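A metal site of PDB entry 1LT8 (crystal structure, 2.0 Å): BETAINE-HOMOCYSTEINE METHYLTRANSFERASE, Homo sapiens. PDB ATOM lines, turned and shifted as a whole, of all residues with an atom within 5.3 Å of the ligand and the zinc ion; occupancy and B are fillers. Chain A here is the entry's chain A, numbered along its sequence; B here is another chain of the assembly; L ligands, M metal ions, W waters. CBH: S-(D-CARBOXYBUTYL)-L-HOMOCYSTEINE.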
ATOM      1  N   GLY A  27     -10.255 -20.016  -4.372  1.00  0.00           N
ATOM      2  CA  GLY A  27     -10.835 -20.659  -3.205  1.00  0.00           C
ATOM      3  C   GLY A  27     -10.311 -22.002  -2.706  1.00  0.00           C
ATOM      4  O   GLY A  27      -9.145 -22.340  -2.909  1.00  0.00           O
ATOM      5  N   GLY A  28     -11.206 -22.745  -2.041  1.00  0.00           N
ATOM      6  CA  GLY A  28     -10.860 -24.045  -1.488  1.00  0.00           C
ATOM      7  C   GLY A  28     -11.308 -25.168  -2.419  1.00  0.00           C
ATOM      8  O   GLY A  28     -12.473 -25.573  -2.396  1.00  0.00           O
ATOM      9  N   PHE A  29     -10.367 -25.665  -3.204  1.00  0.00           N
ATOM     10  CA  PHE A  29     -10.626 -26.725  -4.178  1.00  0.00           C
ATOM     11  C   PHE A  29     -11.090 -28.073  -3.660  1.00  0.00           C
ATOM     12  O   PHE A  29     -12.132 -28.583  -4.106  1.00  0.00           O
ATOM     13  CB  PHE A  29      -9.396 -26.945  -5.064  1.00  0.00           C
ATOM     14  CG  PHE A  29      -9.384 -26.092  -6.294  1.00  0.00           C
ATOM     15  CD1 PHE A  29      -9.259 -24.712  -6.193  1.00  0.00           C
ATOM     16  CD2 PHE A  29      -9.548 -26.669  -7.552  1.00  0.00           C
ATOM     17  CE1 PHE A  29      -9.309 -23.906  -7.331  1.00  0.00           C
ATOM     18  CE2 PHE A  29      -9.602 -25.876  -8.696  1.00  0.00           C
ATOM     19  CZ  PHE A  29      -9.480 -24.493  -8.582  1.00  0.00           C
ATOM     20  N   VAL A  30     -10.342 -28.684  -2.742  1.00  0.00           N
ATOM     21  CA  VAL A  30     -10.730 -30.010  -2.256  1.00  0.00           C
ATOM     22  C   VAL A  30     -12.127 -30.024  -1.671  1.00  0.00           C
ATOM     23  O   VAL A  30     -12.906 -30.929  -1.946  1.00  0.00           O
ATOM     24  CB  VAL A  30      -9.714 -30.574  -1.219  1.00  0.00           C
ATOM     25  CG1 VAL A  30      -8.363 -30.846  -1.897  1.00  0.00           C
ATOM     26  CG2 VAL A  30      -9.548 -29.625  -0.052  1.00  0.00           C
ATOM     27  N   PHE A  31     -12.452 -29.027  -0.862  1.00  0.00           N
ATOM     28  CA  PHE A  31     -13.772 -28.954  -0.255  1.00  0.00           C
ATOM     29  C   PHE A  31     -14.841 -28.688  -1.302  1.00  0.00           C
ATOM     30  O   PHE A  31     -15.913 -29.278  -1.272  1.00  0.00           O
ATOM     31  CB  PHE A  31     -13.814 -27.864   0.821  1.00  0.00           C
ATOM     32  CG  PHE A  31     -13.541 -28.368   2.215  1.00  0.00           C
ATOM     33  CD1 PHE A  31     -14.503 -28.227   3.208  1.00  0.00           C
ATOM     34  CD2 PHE A  31     -12.335 -28.963   2.532  1.00  0.00           C
ATOM     35  CE1 PHE A  31     -14.262 -28.677   4.495  1.00  0.00           C
ATOM     36  CE2 PHE A  31     -12.079 -29.420   3.824  1.00  0.00           C
ATOM     37  CZ  PHE A  31     -13.047 -29.272   4.807  1.00  0.00           C
ATOM     38  N   GLY A  42     -11.100 -37.058   3.579  1.00  0.00           N
ATOM     39  CA  GLY A  42     -10.292 -38.020   4.294  1.00  0.00           C
ATOM     40  C   GLY A  42      -8.899 -37.878   3.734  1.00  0.00           C
ATOM     41  O   GLY A  42      -8.060 -37.183   4.317  1.00  0.00           O
ATOM     42  N   TRP A  44      -8.296 -36.486   0.879  1.00  0.00           N
ATOM     43  CA  TRP A  44      -8.347 -35.208   0.177  1.00  0.00           C
ATOM     44  C   TRP A  44      -7.316 -35.096  -0.964  1.00  0.00           C
ATOM     45  O   TRP A  44      -6.598 -34.094  -1.048  1.00  0.00           O
ATOM     46  CB  TRP A  44      -8.086 -34.056   1.147  1.00  0.00           C
ATOM     47  CG  TRP A  44      -8.995 -33.988   2.338  1.00  0.00           C
ATOM     48  CD1 TRP A  44      -8.660 -34.235   3.649  1.00  0.00           C
ATOM     49  CD2 TRP A  44     -10.356 -33.538   2.362  1.00  0.00           C
ATOM     50  NE1 TRP A  44      -9.722 -33.948   4.478  1.00  0.00           N
ATOM     51  CE2 TRP A  44     -10.770 -33.520   3.714  1.00  0.00           C
ATOM     52  CE3 TRP A  44     -11.259 -33.128   1.361  1.00  0.00           C
ATOM     53  CZ2 TRP A  44     -12.061 -33.116   4.089  1.00  0.00           C
ATOM     54  CZ3 TRP A  44     -12.530 -32.728   1.750  1.00  0.00           C
ATOM     55  CH2 TRP A  44     -12.921 -32.719   3.101  1.00  0.00           C
ATOM     56  N   GLN A  72      -4.212 -21.674  -8.313  1.00  0.00           N
ATOM     57  CA  GLN A  72      -3.279 -22.591  -7.645  1.00  0.00           C
ATOM     58  C   GLN A  72      -3.414 -23.956  -8.299  1.00  0.00           C
ATOM     59  O   GLN A  72      -4.530 -24.384  -8.622  1.00  0.00           O
ATOM     60  CB  GLN A  72      -3.606 -22.707  -6.150  1.00  0.00           C
ATOM     61  CG  GLN A  72      -3.261 -21.487  -5.330  1.00  0.00           C
ATOM     62  CD  GLN A  72      -3.432 -21.717  -3.827  1.00  0.00           C
ATOM     63  OE1 GLN A  72      -2.899 -22.676  -3.279  1.00  0.00           O
ATOM     64  NE2 GLN A  72      -4.174 -20.836  -3.179  1.00  0.00           N
ATOM     65  N   PHE A  76      -2.700 -30.235  -3.963  1.00  0.00           N
ATOM     66  CA  PHE A  76      -2.678 -30.374  -2.517  1.00  0.00           C
ATOM     67  C   PHE A  76      -2.643 -31.878  -2.252  1.00  0.00           C
ATOM     68  O   PHE A  76      -3.454 -32.631  -2.787  1.00  0.00           O
ATOM     69  CB  PHE A  76      -3.947 -29.739  -1.917  1.00  0.00           C
ATOM     70  CG  PHE A  76      -4.062 -29.903  -0.423  1.00  0.00           C
ATOM     71  CD1 PHE A  76      -4.923 -30.846   0.120  1.00  0.00           C
ATOM     72  CD2 PHE A  76      -3.316 -29.094   0.433  1.00  0.00           C
ATOM     73  CE1 PHE A  76      -5.062 -30.997   1.503  1.00  0.00           C
ATOM     74  CE2 PHE A  76      -3.427 -29.240   1.821  1.00  0.00           C
ATOM     75  CZ  PHE A  76      -4.308 -30.188   2.353  1.00  0.00           C
ATOM     76  N   TYR A  77      -1.691 -32.324  -1.432  1.00  0.00           N
ATOM     77  CA  TYR A  77      -1.558 -33.741  -1.148  1.00  0.00           C
ATOM     78  C   TYR A  77      -1.270 -34.485  -2.454  1.00  0.00           C
ATOM     79  O   TYR A  77      -1.744 -35.600  -2.667  1.00  0.00           O
ATOM     80  CB  TYR A  77      -2.860 -34.294  -0.535  1.00  0.00           C
ATOM     81  CG  TYR A  77      -3.080 -33.923   0.914  1.00  0.00           C
ATOM     82  CD1 TYR A  77      -2.196 -33.077   1.595  1.00  0.00           C
ATOM     83  CD2 TYR A  77      -4.180 -34.433   1.617  1.00  0.00           C
ATOM     84  CE1 TYR A  77      -2.394 -32.759   2.934  1.00  0.00           C
ATOM     85  CE2 TYR A  77      -4.391 -34.117   2.954  1.00  0.00           C
ATOM     86  CZ  TYR A  77      -3.496 -33.274   3.616  1.00  0.00           C
ATOM     87  OH  TYR A  77      -3.704 -32.961   4.939  1.00  0.00           O
ATOM     88  N   GLU A 159       2.175 -23.933   1.346  1.00  0.00           N
ATOM     89  CA  GLU A 159       1.034 -23.766   2.226  1.00  0.00           C
ATOM     90  C   GLU A 159       0.723 -24.977   3.083  1.00  0.00           C
ATOM     91  O   GLU A 159       1.292 -26.055   2.917  1.00  0.00           O
ATOM     92  CB  GLU A 159      -0.216 -23.376   1.445  1.00  0.00           C
ATOM     93  CG  GLU A 159      -0.454 -24.213   0.216  1.00  0.00           C
ATOM     94  CD  GLU A 159      -1.863 -24.043  -0.320  1.00  0.00           C
ATOM     95  OE1 GLU A 159      -2.357 -22.893  -0.373  1.00  0.00           O
ATOM     96  OE2 GLU A 159      -2.471 -25.059  -0.710  1.00  0.00           O
ATOM     97  N   TYR A 160      -0.195 -24.763   4.013  1.00  0.00           N
ATOM     98  CA  TYR A 160      -0.620 -25.805   4.942  1.00  0.00           C
ATOM     99  C   TYR A 160       0.584 -26.429   5.628  1.00  0.00           C
ATOM    100  O   TYR A 160       1.001 -27.541   5.300  1.00  0.00           O
ATOM    101  CB  TYR A 160      -1.446 -26.872   4.217  1.00  0.00           C
ATOM    102  CG  TYR A 160      -2.400 -27.579   5.156  1.00  0.00           C
ATOM    103  CD1 TYR A 160      -2.156 -28.891   5.570  1.00  0.00           C
ATOM    104  CD2 TYR A 160      -3.516 -26.918   5.660  1.00  0.00           C
ATOM    105  CE1 TYR A 160      -3.008 -29.521   6.480  1.00  0.00           C
ATOM    106  CE2 TYR A 160      -4.375 -27.541   6.560  1.00  0.00           C
ATOM    107  CZ  TYR A 160      -4.109 -28.851   6.971  1.00  0.00           C
ATOM    108  OH  TYR A 160      -4.960 -29.465   7.863  1.00  0.00           O
ATOM    109  N   ASN A 216      -3.041 -19.745   6.304  1.00  0.00           N
ATOM    110  CA  ASN A 216      -4.111 -20.330   5.506  1.00  0.00           C
ATOM    111  C   ASN A 216      -4.761 -21.490   6.260  1.00  0.00           C
ATOM    112  O   ASN A 216      -4.100 -22.197   7.030  1.00  0.00           O
ATOM    113  CB  ASN A 216      -3.623 -20.779   4.127  1.00  0.00           C
ATOM    114  CG  ASN A 216      -2.997 -22.186   4.122  1.00  0.00           C
ATOM    115  OD1 ASN A 216      -1.906 -22.395   4.644  1.00  0.00           O
ATOM    116  ND2 ASN A 216      -3.697 -23.146   3.529  1.00  0.00           N
ATOM    117  N   CYS A 217      -6.064 -21.640   6.073  1.00  0.00           N
ATOM    118  CA  CYS A 217      -6.818 -22.742   6.681  1.00  0.00           C
ATOM    119  C   CYS A 217      -6.905 -22.709   8.208  1.00  0.00           C
ATOM    120  O   CYS A 217      -6.525 -21.731   8.857  1.00  0.00           O
ATOM    121  CB  CYS A 217      -6.211 -24.060   6.217  1.00  0.00           C
ATOM    122  SG  CYS A 217      -7.387 -25.455   6.167  1.00  0.00           S
ATOM    123  N   HIS A 218      -7.438 -23.792   8.788  1.00  0.00           N
ATOM    124  CA  HIS A 218      -7.569 -23.936  10.238  1.00  0.00           C
ATOM    125  C   HIS A 218      -8.502 -22.991  10.991  1.00  0.00           C
ATOM    126  O   HIS A 218      -9.230 -23.456  11.881  1.00  0.00           O
ATOM    127  CB  HIS A 218      -6.174 -23.876  10.886  1.00  0.00           C
ATOM    128  CG  HIS A 218      -5.467 -25.184  10.909  1.00  0.00           C
ATOM    129  ND1 HIS A 218      -5.520 -26.099   9.878  1.00  0.00           N
ATOM    130  CD2 HIS A 218      -4.630 -25.722  11.833  1.00  0.00           C
ATOM    131  CE1 HIS A 218      -4.760 -27.137  10.154  1.00  0.00           C
ATOM    132  NE2 HIS A 218      -4.207 -26.936  11.335  1.00  0.00           N
ATOM    133  N   LEU A 249     -10.330 -19.933   6.395  1.00  0.00           N
ATOM    134  CA  LEU A 249     -11.466 -20.797   6.119  1.00  0.00           C
ATOM    135  C   LEU A 249     -12.641 -19.869   5.888  1.00  0.00           C
ATOM    136  O   LEU A 249     -12.632 -18.717   6.357  1.00  0.00           O
ATOM    137  CB  LEU A 249     -11.803 -21.658   7.342  1.00  0.00           C
ATOM    138  CG  LEU A 249     -10.768 -22.636   7.876  1.00  0.00           C
ATOM    139  CD1 LEU A 249     -11.250 -23.204   9.228  1.00  0.00           C
ATOM    140  CD2 LEU A 249     -10.552 -23.736   6.849  1.00  0.00           C
ATOM    141  N   PHE A 261      -9.914 -26.010  13.010  1.00  0.00           N
ATOM    142  CA  PHE A 261     -11.227 -26.613  12.832  1.00  0.00           C
ATOM    143  C   PHE A 261     -11.267 -28.134  12.705  1.00  0.00           C
ATOM    144  O   PHE A 261     -12.309 -28.736  12.893  1.00  0.00           O
ATOM    145  CB  PHE A 261     -11.974 -25.968  11.656  1.00  0.00           C
ATOM    146  CG  PHE A 261     -11.553 -26.454  10.283  1.00  0.00           C
ATOM    147  CD1 PHE A 261     -12.479 -26.492   9.235  1.00  0.00           C
ATOM    148  CD2 PHE A 261     -10.235 -26.833  10.005  1.00  0.00           C
ATOM    149  CE1 PHE A 261     -12.119 -26.892   7.950  1.00  0.00           C
ATOM    150  CE2 PHE A 261      -9.857 -27.219   8.728  1.00  0.00           C
ATOM    151  CZ  PHE A 261     -10.799 -27.256   7.691  1.00  0.00           C
ATOM    152  N   ILE A 262     -10.137 -28.767  12.406  1.00  0.00           N
ATOM    153  CA  ILE A 262     -10.130 -30.211  12.275  1.00  0.00           C
ATOM    154  C   ILE A 262     -10.564 -30.903  13.560  1.00  0.00           C
ATOM    155  O   ILE A 262     -11.223 -31.938  13.517  1.00  0.00           O
ATOM    156  CB  ILE A 262      -8.731 -30.728  11.851  1.00  0.00           C
ATOM    157  CG1 ILE A 262      -8.482 -30.346  10.387  1.00  0.00           C
ATOM    158  CG2 ILE A 262      -8.652 -32.235  12.037  1.00  0.00           C
ATOM    159  CD1 ILE A 262      -7.125 -30.748   9.856  1.00  0.00           C
ATOM    160  N   PHE A 267     -16.109 -31.367  11.865  1.00  0.00           N
ATOM    161  CA  PHE A 267     -15.203 -31.526  10.729  1.00  0.00           C
ATOM    162  C   PHE A 267     -15.251 -32.974  10.253  1.00  0.00           C
ATOM    163  O   PHE A 267     -15.118 -33.897  11.064  1.00  0.00           O
ATOM    164  CB  PHE A 267     -13.754 -31.210  11.115  1.00  0.00           C
ATOM    165  CG  PHE A 267     -12.771 -31.444   9.976  1.00  0.00           C
ATOM    166  CD1 PHE A 267     -12.466 -30.419   9.081  1.00  0.00           C
ATOM    167  CD2 PHE A 267     -12.170 -32.699   9.794  1.00  0.00           C
ATOM    168  CE1 PHE A 267     -11.587 -30.637   8.018  1.00  0.00           C
ATOM    169  CE2 PHE A 267     -11.296 -32.929   8.725  1.00  0.00           C
ATOM    170  CZ  PHE A 267     -10.996 -31.891   7.841  1.00  0.00           C
ATOM    171  N   CYS A 299      -9.432 -20.340   1.824  1.00  0.00           N
ATOM    172  CA  CYS A 299      -9.121 -21.747   1.791  1.00  0.00           C
ATOM    173  C   CYS A 299     -10.419 -22.537   1.870  1.00  0.00           C
ATOM    174  O   CYS A 299     -11.436 -22.109   1.319  1.00  0.00           O
ATOM    175  CB  CYS A 299      -8.199 -22.074   2.965  1.00  0.00           C
ATOM    176  SG  CYS A 299      -7.343 -23.642   2.772  1.00  0.00           S
ATOM    177  N   CYS A 300     -10.395 -23.676   2.560  1.00  0.00           N
ATOM    178  CA  CYS A 300     -11.587 -24.514   2.695  1.00  0.00           C
ATOM    179  C   CYS A 300     -12.854 -23.754   3.033  1.00  0.00           C
ATOM    180  O   CYS A 300     -12.901 -23.017   4.010  1.00  0.00           O
ATOM    181  CB  CYS A 300     -11.379 -25.552   3.776  1.00  0.00           C
ATOM    182  SG  CYS A 300      -9.891 -26.513   3.442  1.00  0.00           S
ATOM    183  N   HIS B 338      -7.673 -41.213   8.538  1.00  0.00           N
ATOM    184  CA  HIS B 338      -7.120 -39.910   8.901  1.00  0.00           C
ATOM    185  C   HIS B 338      -6.117 -40.059  10.042  1.00  0.00           C
ATOM    186  O   HIS B 338      -6.208 -40.980  10.838  1.00  0.00           O
ATOM    187  CB  HIS B 338      -8.241 -38.964   9.345  1.00  0.00           C
ATOM    188  CG  HIS B 338      -7.802 -37.541   9.524  1.00  0.00           C
ATOM    189  ND1 HIS B 338      -7.883 -36.606   8.515  1.00  0.00           N
ATOM    190  CD2 HIS B 338      -7.293 -36.885  10.594  1.00  0.00           C
ATOM    191  CE1 HIS B 338      -7.440 -35.442   8.955  1.00  0.00           C
ATOM    192  NE2 HIS B 338      -7.075 -35.585  10.215  1.00  0.00           N
HETATM  193  O11 CBH L   1      -7.628 -25.200  -2.227  1.00  0.00           O
HETATM  194  C12 CBH L   1      -7.310 -26.205  -1.548  1.00  0.00           C
HETATM  195  O13 CBH L   1      -8.058 -27.166  -1.271  1.00  0.00           O
HETATM  196  C14 CBH L   1      -5.855 -26.280  -1.022  1.00  0.00           C
HETATM  197  N15 CBH L   1      -5.048 -25.234  -1.672  1.00  0.00           N
HETATM  198  C16 CBH L   1      -5.807 -26.087   0.504  1.00  0.00           C
HETATM  199  C17 CBH L   1      -6.449 -27.262   1.233  1.00  0.00           C
HETATM  200  S18 CBH L   1      -6.282 -27.182   3.060  1.00  0.00           S
HETATM  201  C19 CBH L   1      -7.145 -28.750   3.450  1.00  0.00           C
HETATM  202  C20 CBH L   1      -7.022 -29.165   4.902  1.00  0.00           C
HETATM  203  C21 CBH L   1      -7.456 -30.622   5.064  1.00  0.00           C
HETATM  204  C22 CBH L   1      -7.156 -31.122   6.463  1.00  0.00           C
HETATM  205  C23 CBH L   1      -7.228 -32.648   6.508  1.00  0.00           C
HETATM  206  O25 CBH L   1      -6.203 -33.269   6.175  1.00  0.00           O
HETATM  207  O24 CBH L   1      -8.304 -33.154   6.860  1.00  0.00           O
HETATM  208 ZN    ZN M   1      -7.800 -25.635   3.889  1.00  0.00          ZN
HETATM  209  O   HOH W   1      -4.941 -26.406  -4.566  1.00  0.00           O
HETATM  210  O   HOH W   2      -3.687 -25.625   2.626  1.00  0.00           O
HETATM  211  O   HOH W   3     -10.510 -26.676   0.048  1.00  0.00           O
HETATM  212  O   HOH W   4      -6.457 -23.306  -4.077  1.00  0.00           O
HETATM  213  O   HOH W   5      -5.634 -36.099   5.716  1.00  0.00           O
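Water W4 lies within hydrogen-bond range of O11 of the ligand, O of Gly 27 and NE2 of Gln 72.
Water W5 bridges an oxygen (O25) of the ligand (2.9 Å) and the backbone carbonyl oxygen (O) of Gly 42 (3.0 Å).
The side-chain sulfur (SG) of Cys 299 lies close to the side-chain amide nitrogen (ND2) of Asn 216.
O of Cys 299 lies within hydrogen-bond range of N of Gly 28 (3.4 Å).
OE1 of Gln 72 sits close to OE1 of Glu 159 (3.0 Å).
OD1 of Asn 216 sits at hydrogen-bond distance from N of Tyr 160.
The zinc ion is bound by SG of Cys 300 (2.3 Å), S18 of the ligand (2.3 Å), SG of Cys 217 (2.3 Å) and SG of Cys 299 (2.3 Å).
The backbone NH of Phe 29 sits at hydrogen-bond distance from an oxygen (O11) of the ligand (2.9 Å).
The side-chain hydroxyl (OH) of Tyr 77 is in hydrogen-bond range of an oxygen (O25) of the ligand (2.8 Å).
The indole nitrogen (NE1) of Trp 44 sits at hydrogen-bond distance from an oxygen (O24) of the ligand, 2.9 Å away.
OE2 of Glu 159 is in salt-bridge range of N15 of the ligand (2.8 Å).
N of Val 30 lies within hydrogen-bond range of O13 of the ligand (3.1 Å).
O of Gly 27 sits close to O11 of the ligand, at 3.3 Å.
Gly 28 touches the ligand (CA to O11, 3.5 Å).
Gln 72 touches the ligand (OE1 to N15, 3.7 Å).
CZ of Phe 76 touches C19 of the ligand, 3.4 Å away.
Tyr 160 touches the ligand.
Ile 262 touches the ligand.
Phe 267 touches the ligand (CZ to O24, 3.1 Å).
CE1 of His 338 of chain B touches O24 of the ligand, at 3.2 Å.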
